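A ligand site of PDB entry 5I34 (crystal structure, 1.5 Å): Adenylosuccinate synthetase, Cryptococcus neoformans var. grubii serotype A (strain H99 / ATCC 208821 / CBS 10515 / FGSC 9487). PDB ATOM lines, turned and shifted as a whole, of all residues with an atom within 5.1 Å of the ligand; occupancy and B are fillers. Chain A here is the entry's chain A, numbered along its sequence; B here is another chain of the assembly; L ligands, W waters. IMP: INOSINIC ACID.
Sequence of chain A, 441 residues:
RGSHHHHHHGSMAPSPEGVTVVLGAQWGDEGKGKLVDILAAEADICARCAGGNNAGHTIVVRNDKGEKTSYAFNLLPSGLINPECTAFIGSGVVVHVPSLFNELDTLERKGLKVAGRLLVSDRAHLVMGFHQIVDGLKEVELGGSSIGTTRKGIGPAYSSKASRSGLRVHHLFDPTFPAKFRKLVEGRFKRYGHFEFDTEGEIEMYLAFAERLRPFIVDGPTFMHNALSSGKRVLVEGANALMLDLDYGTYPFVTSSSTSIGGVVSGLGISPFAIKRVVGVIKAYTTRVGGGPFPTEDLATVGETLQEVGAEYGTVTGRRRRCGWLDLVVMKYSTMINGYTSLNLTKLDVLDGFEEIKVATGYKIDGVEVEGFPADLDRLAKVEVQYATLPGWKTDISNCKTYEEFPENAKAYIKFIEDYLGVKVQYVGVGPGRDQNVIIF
The guanidinium group of Arg 164 of chain B lies within salt-bridge range of an oxygen (O1P) of the ligand (2.9 Å). O of Gly 148 is in hydrogen-bond range of O2' of the ligand (3.2 Å). The side-chain hydroxyl (OG1) of Thr 150 is in hydrogen-bond range of an oxygen (O2P) of the ligand (2.6 Å). An oxygen (O3') of the ligand sits at hydrogen-bond distance from the backbone carbonyl oxygen (O) of Ile 147 (3.2 Å). OG1 of Thr 255 is in hydrogen-bond range of O3P of the ligand, at 2.7 Å. The guanidinium group (NH2) of Arg 319 is in hydrogen-bond range of an oxygen (O2') of the ligand, at 2.5 Å. A nitrogen (N7) of the ligand lies within hydrogen-bond range of the side-chain amide nitrogen (ND2) of Asn 240, at 2.9 Å. The side-chain carboxylate (OD2) of Asp 29 sits at hydrogen-bond distance from a nitrogen (N1) of the ligand (3.3 Å). An oxygen (O2') of the ligand sits at hydrogen-bond distance from the backbone carbonyl oxygen (O) of Val 289, 3.0 Å away. The backbone NH (N) of Thr 150 lies within hydrogen-bond range of an oxygen (O2P) of the ligand (2.7 Å).
The side-chain hydroxyl of Thr 150 lies within hydrogen-bond range of the side-chain amide nitrogen of Asn 54 (2.8 Å). NE of Arg 164 of chain B lies close to OG of Ser 256, 3.3 Å away. OG1 of Thr 149 sits at hydrogen-bond distance from OD1 of Asp 135 (2.8 Å). OG1 of Thr 149 sits close to N of Arg 151, at 3.3 Å. The side-chain amide oxygen (OD1) of Asn 54 sits at hydrogen-bond distance from the side-chain amino group (NZ) of Lys 152, 3.1 Å away. N of Thr 255 is in hydrogen-bond range of O of Leu 244. The backbone carbonyl oxygen (O) of Val 254 is in hydrogen-bond range of the guanidinium group (NH2) of Arg 164 of chain B. The guanidinium group (NH1) of Arg 319 sits at hydrogen-bond distance from the backbone carbonyl oxygen (O) of Gly 148, 2.8 Å away.
Merely in contact with the ligand: Trp 27 (3.4 Å), Gly 28 (3.99 Å), Asn 54 (3.5 Å), Thr 149 (3.4 Å), Leu 244 (3.4 Å) and Val 254 (3.2 Å). Hydrophobic or aromatic side chains that line the ligand: Ile 147, Leu 244 and Val 289. Along chain A the residues within 4 Å of the ligand span positions 27 to 319.
Water W4 lies within hydrogen-bond range of an oxygen (O3P) of the ligand (2.6 Å), the side-chain amide nitrogen (ND2) of Asn 54 (2.8 Å), the side-chain amide nitrogen (ND2) of Asn 240 (3.2 Å) and the side-chain hydroxyl (OG1) of Thr 255 (3.4 Å). Water W1 lies within hydrogen-bond range of O1P of the ligand (2.7 Å), NH1 of Arg 164 of chain B (2.9 Å), N of Gly 155 (3.0 Å) and OD1 of Asp 135 (3.1 Å). Water W2 lies within hydrogen-bond range of an oxygen (O1P) of the ligand (2.8 Å), the side-chain hydroxyl (OG) of Ser 256 (2.8 Å), the side-chain hydroxyl (OG1) of Thr 255 (3.2 Å), the backbone NH (N) of Gly 155 (3.2 Å) and the guanidinium group (NH2) of Arg 164 of chain B (3.2 Å). Water W3 lies within hydrogen-bond range of OD2 of Asp 135, O2P of the ligand, N of Lys 152, N of Ile 154 and OG1 of Thr 150.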
ATOM      1  N   TRP A  27      20.512  -7.466 -24.557  1.00  0.00           N
ATOM      2  CA  TRP A  27      19.099  -7.724 -24.865  1.00  0.00           C
ATOM      3  C   TRP A  27      18.695  -7.077 -26.200  1.00  0.00           C
ATOM      4  O   TRP A  27      17.553  -6.607 -26.378  1.00  0.00           O
ATOM      5  CB  TRP A  27      18.194  -7.217 -23.745  1.00  0.00           C
ATOM      6  CG  TRP A  27      18.068  -8.082 -22.513  1.00  0.00           C
ATOM      7  CD1 TRP A  27      17.238  -9.152 -22.351  1.00  0.00           C
ATOM      8  CD2 TRP A  27      18.749  -7.920 -21.247  1.00  0.00           C
ATOM      9  NE1 TRP A  27      17.343  -9.661 -21.088  1.00  0.00           N
ATOM     10  CE2 TRP A  27      18.278  -8.922 -20.384  1.00  0.00           C
ATOM     11  CE3 TRP A  27      19.697  -7.016 -20.770  1.00  0.00           C
ATOM     12  CZ2 TRP A  27      18.740  -9.056 -19.079  1.00  0.00           C
ATOM     13  CZ3 TRP A  27      20.152  -7.146 -19.487  1.00  0.00           C
ATOM     14  CH2 TRP A  27      19.675  -8.153 -18.651  1.00  0.00           C
ATOM     15  N   GLY A  28      19.608  -7.045 -27.159  1.00  0.00           N
ATOM     16  CA  GLY A  28      19.272  -6.507 -28.469  1.00  0.00           C
ATOM     17  C   GLY A  28      19.475  -5.013 -28.618  1.00  0.00           C
ATOM     18  O   GLY A  28      19.775  -4.306 -27.648  1.00  0.00           O
ATOM     19  N   ASP A  29      19.327  -4.550 -29.863  1.00  0.00           N
ATOM     20  CA  ASP A  29      19.460  -3.128 -30.160  1.00  0.00           C
ATOM     21  C   ASP A  29      20.838  -2.594 -29.801  1.00  0.00           C
ATOM     22  O   ASP A  29      20.995  -1.402 -29.531  1.00  0.00           O
ATOM     23  CB  ASP A  29      18.370  -2.329 -29.435  1.00  0.00           C
ATOM     24  CG  ASP A  29      16.985  -2.905 -29.669  1.00  0.00           C
ATOM     25  OD1 ASP A  29      16.278  -3.203 -28.691  1.00  0.00           O
ATOM     26  OD2 ASP A  29      16.614  -3.089 -30.854  1.00  0.00           O
ATOM     27  N   ASN A  54      13.402  -9.699 -37.439  1.00  0.00           N
ATOM     28  CA  ASN A  54      13.771  -8.693 -36.446  1.00  0.00           C
ATOM     29  C   ASN A  54      15.259  -8.371 -36.488  1.00  0.00           C
ATOM     30  O   ASN A  54      15.936  -8.312 -35.454  1.00  0.00           O
ATOM     31  CB  ASN A  54      13.376  -9.147 -35.050  1.00  0.00           C
ATOM     32  CG  ASN A  54      11.938  -8.819 -34.714  1.00  0.00           C
ATOM     33  OD1 ASN A  54      11.485  -7.671 -34.893  1.00  0.00           O
ATOM     34  ND2 ASN A  54      11.208  -9.805 -34.235  1.00  0.00           N
ATOM     35  N   ASP A 135       0.201 -14.858 -32.538  1.00  0.00           N
ATOM     36  CA  ASP A 135       1.251 -14.254 -31.713  1.00  0.00           C
ATOM     37  C   ASP A 135       0.586 -13.169 -30.866  1.00  0.00           C
ATOM     38  O   ASP A 135       0.705 -13.140 -29.628  1.00  0.00           O
ATOM     39  CB  ASP A 135       2.351 -13.680 -32.619  1.00  0.00           C
ATOM     40  CG  ASP A 135       3.659 -13.360 -31.908  1.00  0.00           C
ATOM     41  OD1 ASP A 135       3.771 -13.468 -30.669  1.00  0.00           O
ATOM     42  OD2 ASP A 135       4.602 -12.963 -32.640  1.00  0.00           O
ATOM     43  N   ILE A 147       4.732 -11.148 -22.874  1.00  0.00           N
ATOM     44  CA  ILE A 147       6.184 -11.176 -23.078  1.00  0.00           C
ATOM     45  C   ILE A 147       6.715  -9.934 -23.766  1.00  0.00           C
ATOM     46  O   ILE A 147       7.907  -9.609 -23.662  1.00  0.00           O
ATOM     47  CB  ILE A 147       6.579 -12.391 -23.939  1.00  0.00           C
ATOM     48  CG1 ILE A 147       6.413 -13.662 -23.116  1.00  0.00           C
ATOM     49  CG2 ILE A 147       8.010 -12.262 -24.509  1.00  0.00           C
ATOM     50  CD1 ILE A 147       6.724 -14.915 -23.915  1.00  0.00           C
ATOM     51  N   GLY A 148       5.851  -9.260 -24.511  1.00  0.00           N
ATOM     52  CA  GLY A 148       6.269  -8.144 -25.336  1.00  0.00           C
ATOM     53  C   GLY A 148       6.849  -8.585 -26.664  1.00  0.00           C
ATOM     54  O   GLY A 148       7.794  -7.970 -27.168  1.00  0.00           O
ATOM     55  N   THR A 149       6.278  -9.629 -27.262  1.00  0.00           N
ATOM     56  CA  THR A 149       6.769 -10.073 -28.577  1.00  0.00           C
ATOM     57  C   THR A 149       6.549  -8.996 -29.620  1.00  0.00           C
ATOM     58  O   THR A 149       5.718  -8.079 -29.442  1.00  0.00           O
ATOM     59  CB  THR A 149       6.109 -11.361 -29.086  1.00  0.00           C
ATOM     60  OG1 THR A 149       4.780 -11.062 -29.554  1.00  0.00           O
ATOM     61  CG2 THR A 149       6.080 -12.444 -28.008  1.00  0.00           C
ATOM     62  N   THR A 150       7.265  -9.124 -30.729  1.00  0.00           N
ATOM     63  CA  THR A 150       7.156  -8.163 -31.829  1.00  0.00           C
ATOM     64  C   THR A 150       5.935  -8.423 -32.715  1.00  0.00           C
ATOM     65  O   THR A 150       5.681  -7.671 -33.682  1.00  0.00           O
ATOM     66  CB  THR A 150       8.404  -8.192 -32.707  1.00  0.00           C
ATOM     67  OG1 THR A 150       8.592  -9.508 -33.269  1.00  0.00           O
ATOM     68  CG2 THR A 150       9.620  -7.803 -31.877  1.00  0.00           C
ATOM     69  N   ARG A 151       5.189  -9.472 -32.370  1.00  0.00           N
ATOM     70  CA  ARG A 151       3.947  -9.866 -33.053  1.00  0.00           C
ATOM     71  C   ARG A 151       4.185 -10.133 -34.531  1.00  0.00           C
ATOM     72  O   ARG A 151       3.299  -9.906 -35.374  1.00  0.00           O
ATOM     73  CB  ARG A 151       2.871  -8.812 -32.850  1.00  0.00           C
ATOM     74  CG  ARG A 151       2.608  -8.605 -31.372  1.00  0.00           C
ATOM     75  CD  ARG A 151       1.194  -8.271 -31.063  1.00  0.00           C
ATOM     76  NE  ARG A 151       1.018  -8.032 -29.639  1.00  0.00           N
ATOM     77  CZ  ARG A 151      -0.127  -7.645 -29.092  1.00  0.00           C
ATOM     78  NH1 ARG A 151      -1.197  -7.460 -29.857  1.00  0.00           N
ATOM     79  NH2 ARG A 151      -0.204  -7.430 -27.781  1.00  0.00           N
ATOM     80  N   LYS A 152       5.381 -10.653 -34.834  1.00  0.00           N
ATOM     81  CA  LYS A 152       5.730 -11.027 -36.194  1.00  0.00           C
ATOM     82  C   LYS A 152       5.594 -12.525 -36.457  1.00  0.00           C
ATOM     83  O   LYS A 152       6.018 -12.998 -37.503  1.00  0.00           O
ATOM     84  CB  LYS A 152       7.142 -10.570 -36.498  1.00  0.00           C
ATOM     85  CG  LYS A 152       7.251  -9.050 -36.637  1.00  0.00           C
ATOM     86  CD  LYS A 152       8.668  -8.553 -36.861  1.00  0.00           C
ATOM     87  CE  LYS A 152       8.685  -7.060 -37.055  1.00  0.00           C
ATOM     88  NZ  LYS A 152      10.028  -6.501 -37.389  1.00  0.00           N
ATOM     89  N   ILE A 154       6.987 -15.065 -34.898  1.00  0.00           N
ATOM     90  CA  ILE A 154       8.214 -15.852 -34.753  1.00  0.00           C
ATOM     91  C   ILE A 154       8.042 -17.026 -33.790  1.00  0.00           C
ATOM     92  O   ILE A 154       8.413 -18.158 -34.116  1.00  0.00           O
ATOM     93  CB  ILE A 154       9.401 -14.968 -34.276  1.00  0.00           C
ATOM     94  CG1 ILE A 154       9.613 -13.804 -35.246  1.00  0.00           C
ATOM     95  CG2 ILE A 154      10.675 -15.807 -34.081  1.00  0.00           C
ATOM     96  CD1 ILE A 154       9.980 -14.187 -36.580  1.00  0.00           C
ATOM     97  N   GLY A 155       7.461 -16.765 -32.623  1.00  0.00           N
ATOM     98  CA  GLY A 155       7.217 -17.825 -31.655  1.00  0.00           C
ATOM     99  C   GLY A 155       6.311 -18.914 -32.206  1.00  0.00           C
ATOM    100  O   GLY A 155       6.658 -20.097 -32.137  1.00  0.00           O
ATOM    101  N   ASN A 240      18.866 -10.677 -32.978  1.00  0.00           N
ATOM    102  CA  ASN A 240      18.557 -10.508 -31.578  1.00  0.00           C
ATOM    103  C   ASN A 240      19.857 -10.499 -30.764  1.00  0.00           C
ATOM    104  O   ASN A 240      20.856  -9.910 -31.187  1.00  0.00           O
ATOM    105  CB  ASN A 240      17.591 -11.609 -31.138  1.00  0.00           C
ATOM    106  CG  ASN A 240      16.519 -11.908 -32.191  1.00  0.00           C
ATOM    107  OD1 ASN A 240      16.506 -12.960 -32.839  1.00  0.00           O
ATOM    108  ND2 ASN A 240      15.627 -10.963 -32.386  1.00  0.00           N
ATOM    109  N   LEU A 244      18.273 -12.733 -25.019  1.00  0.00           N
ATOM    110  CA  LEU A 244      17.006 -13.136 -25.637  1.00  0.00           C
ATOM    111  C   LEU A 244      17.048 -14.592 -26.129  1.00  0.00           C
ATOM    112  O   LEU A 244      16.095 -15.063 -26.756  1.00  0.00           O
ATOM    113  CB  LEU A 244      16.666 -12.215 -26.810  1.00  0.00           C
ATOM    114  CG  LEU A 244      16.474 -10.757 -26.424  1.00  0.00           C
ATOM    115  CD1 LEU A 244      16.392  -9.883 -27.663  1.00  0.00           C
ATOM    116  CD2 LEU A 244      15.235 -10.566 -25.530  1.00  0.00           C
ATOM    117  N   PHE A 253      10.876 -14.036 -21.205  1.00  0.00           N
ATOM    118  CA  PHE A 253      11.093 -12.807 -21.960  1.00  0.00           C
ATOM    119  C   PHE A 253      12.306 -12.974 -22.866  1.00  0.00           C
ATOM    120  O   PHE A 253      13.364 -12.347 -22.685  1.00  0.00           O
ATOM    121  CB  PHE A 253      11.256 -11.643 -20.989  1.00  0.00           C
ATOM    122  CG  PHE A 253      10.120 -11.542 -20.001  1.00  0.00           C
ATOM    123  CD1 PHE A 253       8.911 -11.000 -20.389  1.00  0.00           C
ATOM    124  CD2 PHE A 253      10.261 -11.997 -18.697  1.00  0.00           C
ATOM    125  CE1 PHE A 253       7.859 -10.915 -19.491  1.00  0.00           C
ATOM    126  CE2 PHE A 253       9.221 -11.916 -17.794  1.00  0.00           C
ATOM    127  CZ  PHE A 253       8.031 -11.365 -18.180  1.00  0.00           C
ATOM    128  N   VAL A 254      12.119 -13.835 -23.858  1.00  0.00           N
ATOM    129  CA  VAL A 254      13.139 -14.232 -24.801  1.00  0.00           C
ATOM    130  C   VAL A 254      12.457 -14.477 -26.142  1.00  0.00           C
ATOM    131  O   VAL A 254      11.214 -14.540 -26.226  1.00  0.00           O
ATOM    132  CB  VAL A 254      13.869 -15.531 -24.344  1.00  0.00           C
ATOM    133  CG1 VAL A 254      14.631 -15.314 -23.025  1.00  0.00           C
ATOM    134  CG2 VAL A 254      12.857 -16.692 -24.207  1.00  0.00           C
ATOM    135  N   THR A 255      13.271 -14.606 -27.192  1.00  0.00           N
ATOM    136  CA  THR A 255      12.764 -15.037 -28.483  1.00  0.00           C
ATOM    137  C   THR A 255      12.874 -16.571 -28.553  1.00  0.00           C
ATOM    138  O   THR A 255      13.407 -17.206 -27.623  1.00  0.00           O
ATOM    139  CB  THR A 255      13.524 -14.331 -29.635  1.00  0.00           C
ATOM    140  OG1 THR A 255      12.834 -14.541 -30.869  1.00  0.00           O
ATOM    141  CG2 THR A 255      14.919 -14.860 -29.760  1.00  0.00           C
ATOM    142  N   SER A 256      12.324 -17.157 -29.611  1.00  0.00           N
ATOM    143  CA  SER A 256      12.119 -18.600 -29.668  1.00  0.00           C
ATOM    144  C   SER A 256      13.162 -19.352 -30.485  1.00  0.00           C
ATOM    145  O   SER A 256      12.930 -20.491 -30.872  1.00  0.00           O
ATOM    146  CB  SER A 256      10.732 -18.880 -30.220  1.00  0.00           C
ATOM    147  OG  SER A 256       9.779 -18.297 -29.352  1.00  0.00           O
ATOM    148  N   VAL A 289      13.743  -4.270 -24.065  1.00  0.00           N
ATOM    149  CA  VAL A 289      12.354  -4.112 -24.453  1.00  0.00           C
ATOM    150  C   VAL A 289      11.599  -5.371 -24.057  1.00  0.00           C
ATOM    151  O   VAL A 289      11.893  -6.457 -24.556  1.00  0.00           O
ATOM    152  CB  VAL A 289      12.206  -3.871 -25.956  1.00  0.00           C
ATOM    153  CG1 VAL A 289      10.730  -3.758 -26.339  1.00  0.00           C
ATOM    154  CG2 VAL A 289      12.959  -2.636 -26.370  1.00  0.00           C
ATOM    155  N   GLY A 290      10.622  -5.226 -23.164  1.00  0.00           N
ATOM    156  CA  GLY A 290       9.847  -6.351 -22.712  1.00  0.00           C
ATOM    157  C   GLY A 290       9.813  -6.398 -21.199  1.00  0.00           C
ATOM    158  O   GLY A 290      10.452  -5.580 -20.536  1.00  0.00           O
ATOM    159  N   ARG A 319       7.192  -0.313 -27.731  1.00  0.00           N
ATOM    160  CA  ARG A 319       8.538  -0.875 -27.686  1.00  0.00           C
ATOM    161  C   ARG A 319       9.611   0.187 -27.439  1.00  0.00           C
ATOM    162  O   ARG A 319      10.782  -0.013 -27.802  1.00  0.00           O
ATOM    163  CB  ARG A 319       8.837  -1.642 -28.979  1.00  0.00           C
ATOM    164  CG  ARG A 319       7.902  -2.846 -29.182  1.00  0.00           C
ATOM    165  CD  ARG A 319       8.319  -3.745 -30.341  1.00  0.00           C
ATOM    166  NE  ARG A 319       9.626  -4.378 -30.144  1.00  0.00           N
ATOM    167  CZ  ARG A 319       9.846  -5.364 -29.278  1.00  0.00           C
ATOM    168  NH1 ARG A 319       8.864  -5.827 -28.519  1.00  0.00           N
ATOM    169  NH2 ARG A 319      11.061  -5.882 -29.159  1.00  0.00           N
ATOM    170  N   ARG B 164       7.212 -20.458 -25.129  1.00  0.00           N
ATOM    171  CA  ARG B 164       7.642 -19.839 -23.866  1.00  0.00           C
ATOM    172  C   ARG B 164       6.552 -19.908 -22.802  1.00  0.00           C
ATOM    173  O   ARG B 164       6.576 -19.183 -21.810  1.00  0.00           O
ATOM    174  CB  ARG B 164       8.124 -18.395 -24.076  1.00  0.00           C
ATOM    175  CG  ARG B 164       9.344 -18.357 -24.959  1.00  0.00           C
ATOM    176  CD  ARG B 164       9.369 -17.109 -25.820  1.00  0.00           C
ATOM    177  NE  ARG B 164       8.221 -17.073 -26.712  1.00  0.00           N
ATOM    178  CZ  ARG B 164       8.019 -16.138 -27.648  1.00  0.00           C
ATOM    179  NH1 ARG B 164       6.949 -16.192 -28.425  1.00  0.00           N
ATOM    180  NH2 ARG B 164       8.898 -15.148 -27.808  1.00  0.00           N
HETATM  181  P   IMP L   1       9.721 -12.166 -30.451  1.00  0.00           P
HETATM  182  O1P IMP L   1       8.952 -13.428 -30.117  1.00  0.00           O
HETATM  183  O2P IMP L   1       8.876 -11.270 -31.330  1.00  0.00           O
HETATM  184  O3P IMP L   1      11.106 -12.528 -30.938  1.00  0.00           O
HETATM  185  O5' IMP L   1       9.912 -11.339 -29.072  1.00  0.00           O
HETATM  186  C5' IMP L   1      10.274 -12.026 -27.883  1.00  0.00           C
HETATM  187  C4' IMP L   1      10.978 -11.140 -26.879  1.00  0.00           C
HETATM  188  O4' IMP L   1      12.280 -10.795 -27.426  1.00  0.00           O
HETATM  189  C3' IMP L   1      10.321  -9.806 -26.543  1.00  0.00           C
HETATM  190  O3' IMP L   1      10.716  -9.414 -25.221  1.00  0.00           O
HETATM  191  C2' IMP L   1      10.955  -8.870 -27.572  1.00  0.00           C
HETATM  192  O2' IMP L   1      10.943  -7.505 -27.247  1.00  0.00           O
HETATM  193  C1' IMP L   1      12.375  -9.403 -27.592  1.00  0.00           C
HETATM  194  N9  IMP L   1      13.050  -9.184 -28.865  1.00  0.00           N
HETATM  195  C8  IMP L   1      12.988  -9.960 -29.988  1.00  0.00           C
HETATM  196  N7  IMP L   1      13.786  -9.368 -30.902  1.00  0.00           N
HETATM  197  C5  IMP L   1      14.326  -8.256 -30.360  1.00  0.00           C
HETATM  198  C6  IMP L   1      15.270  -7.217 -30.917  1.00  0.00           C
HETATM  199  O6  IMP L   1      15.685  -7.317 -32.065  1.00  0.00           O
HETATM  200  N1  IMP L   1      15.646  -6.152 -30.088  1.00  0.00           N
HETATM  201  C2  IMP L   1      15.152  -6.037 -28.748  1.00  0.00           C
HETATM  202  N3  IMP L   1      14.261  -7.021 -28.205  1.00  0.00           N
HETATM  203  C4  IMP L   1      13.859  -8.138 -29.078  1.00  0.00           C
HETATM  204  O   HOH W   1       6.644 -14.524 -30.829  1.00  0.00           O
HETATM  205  O   HOH W   2       9.953 -15.911 -30.769  1.00  0.00           O
HETATM  206  O   HOH W   3       7.121 -12.404 -33.239  1.00  0.00           O
HETATM  207  O   HOH W   4      12.626 -11.835 -32.971  1.00  0.00           O
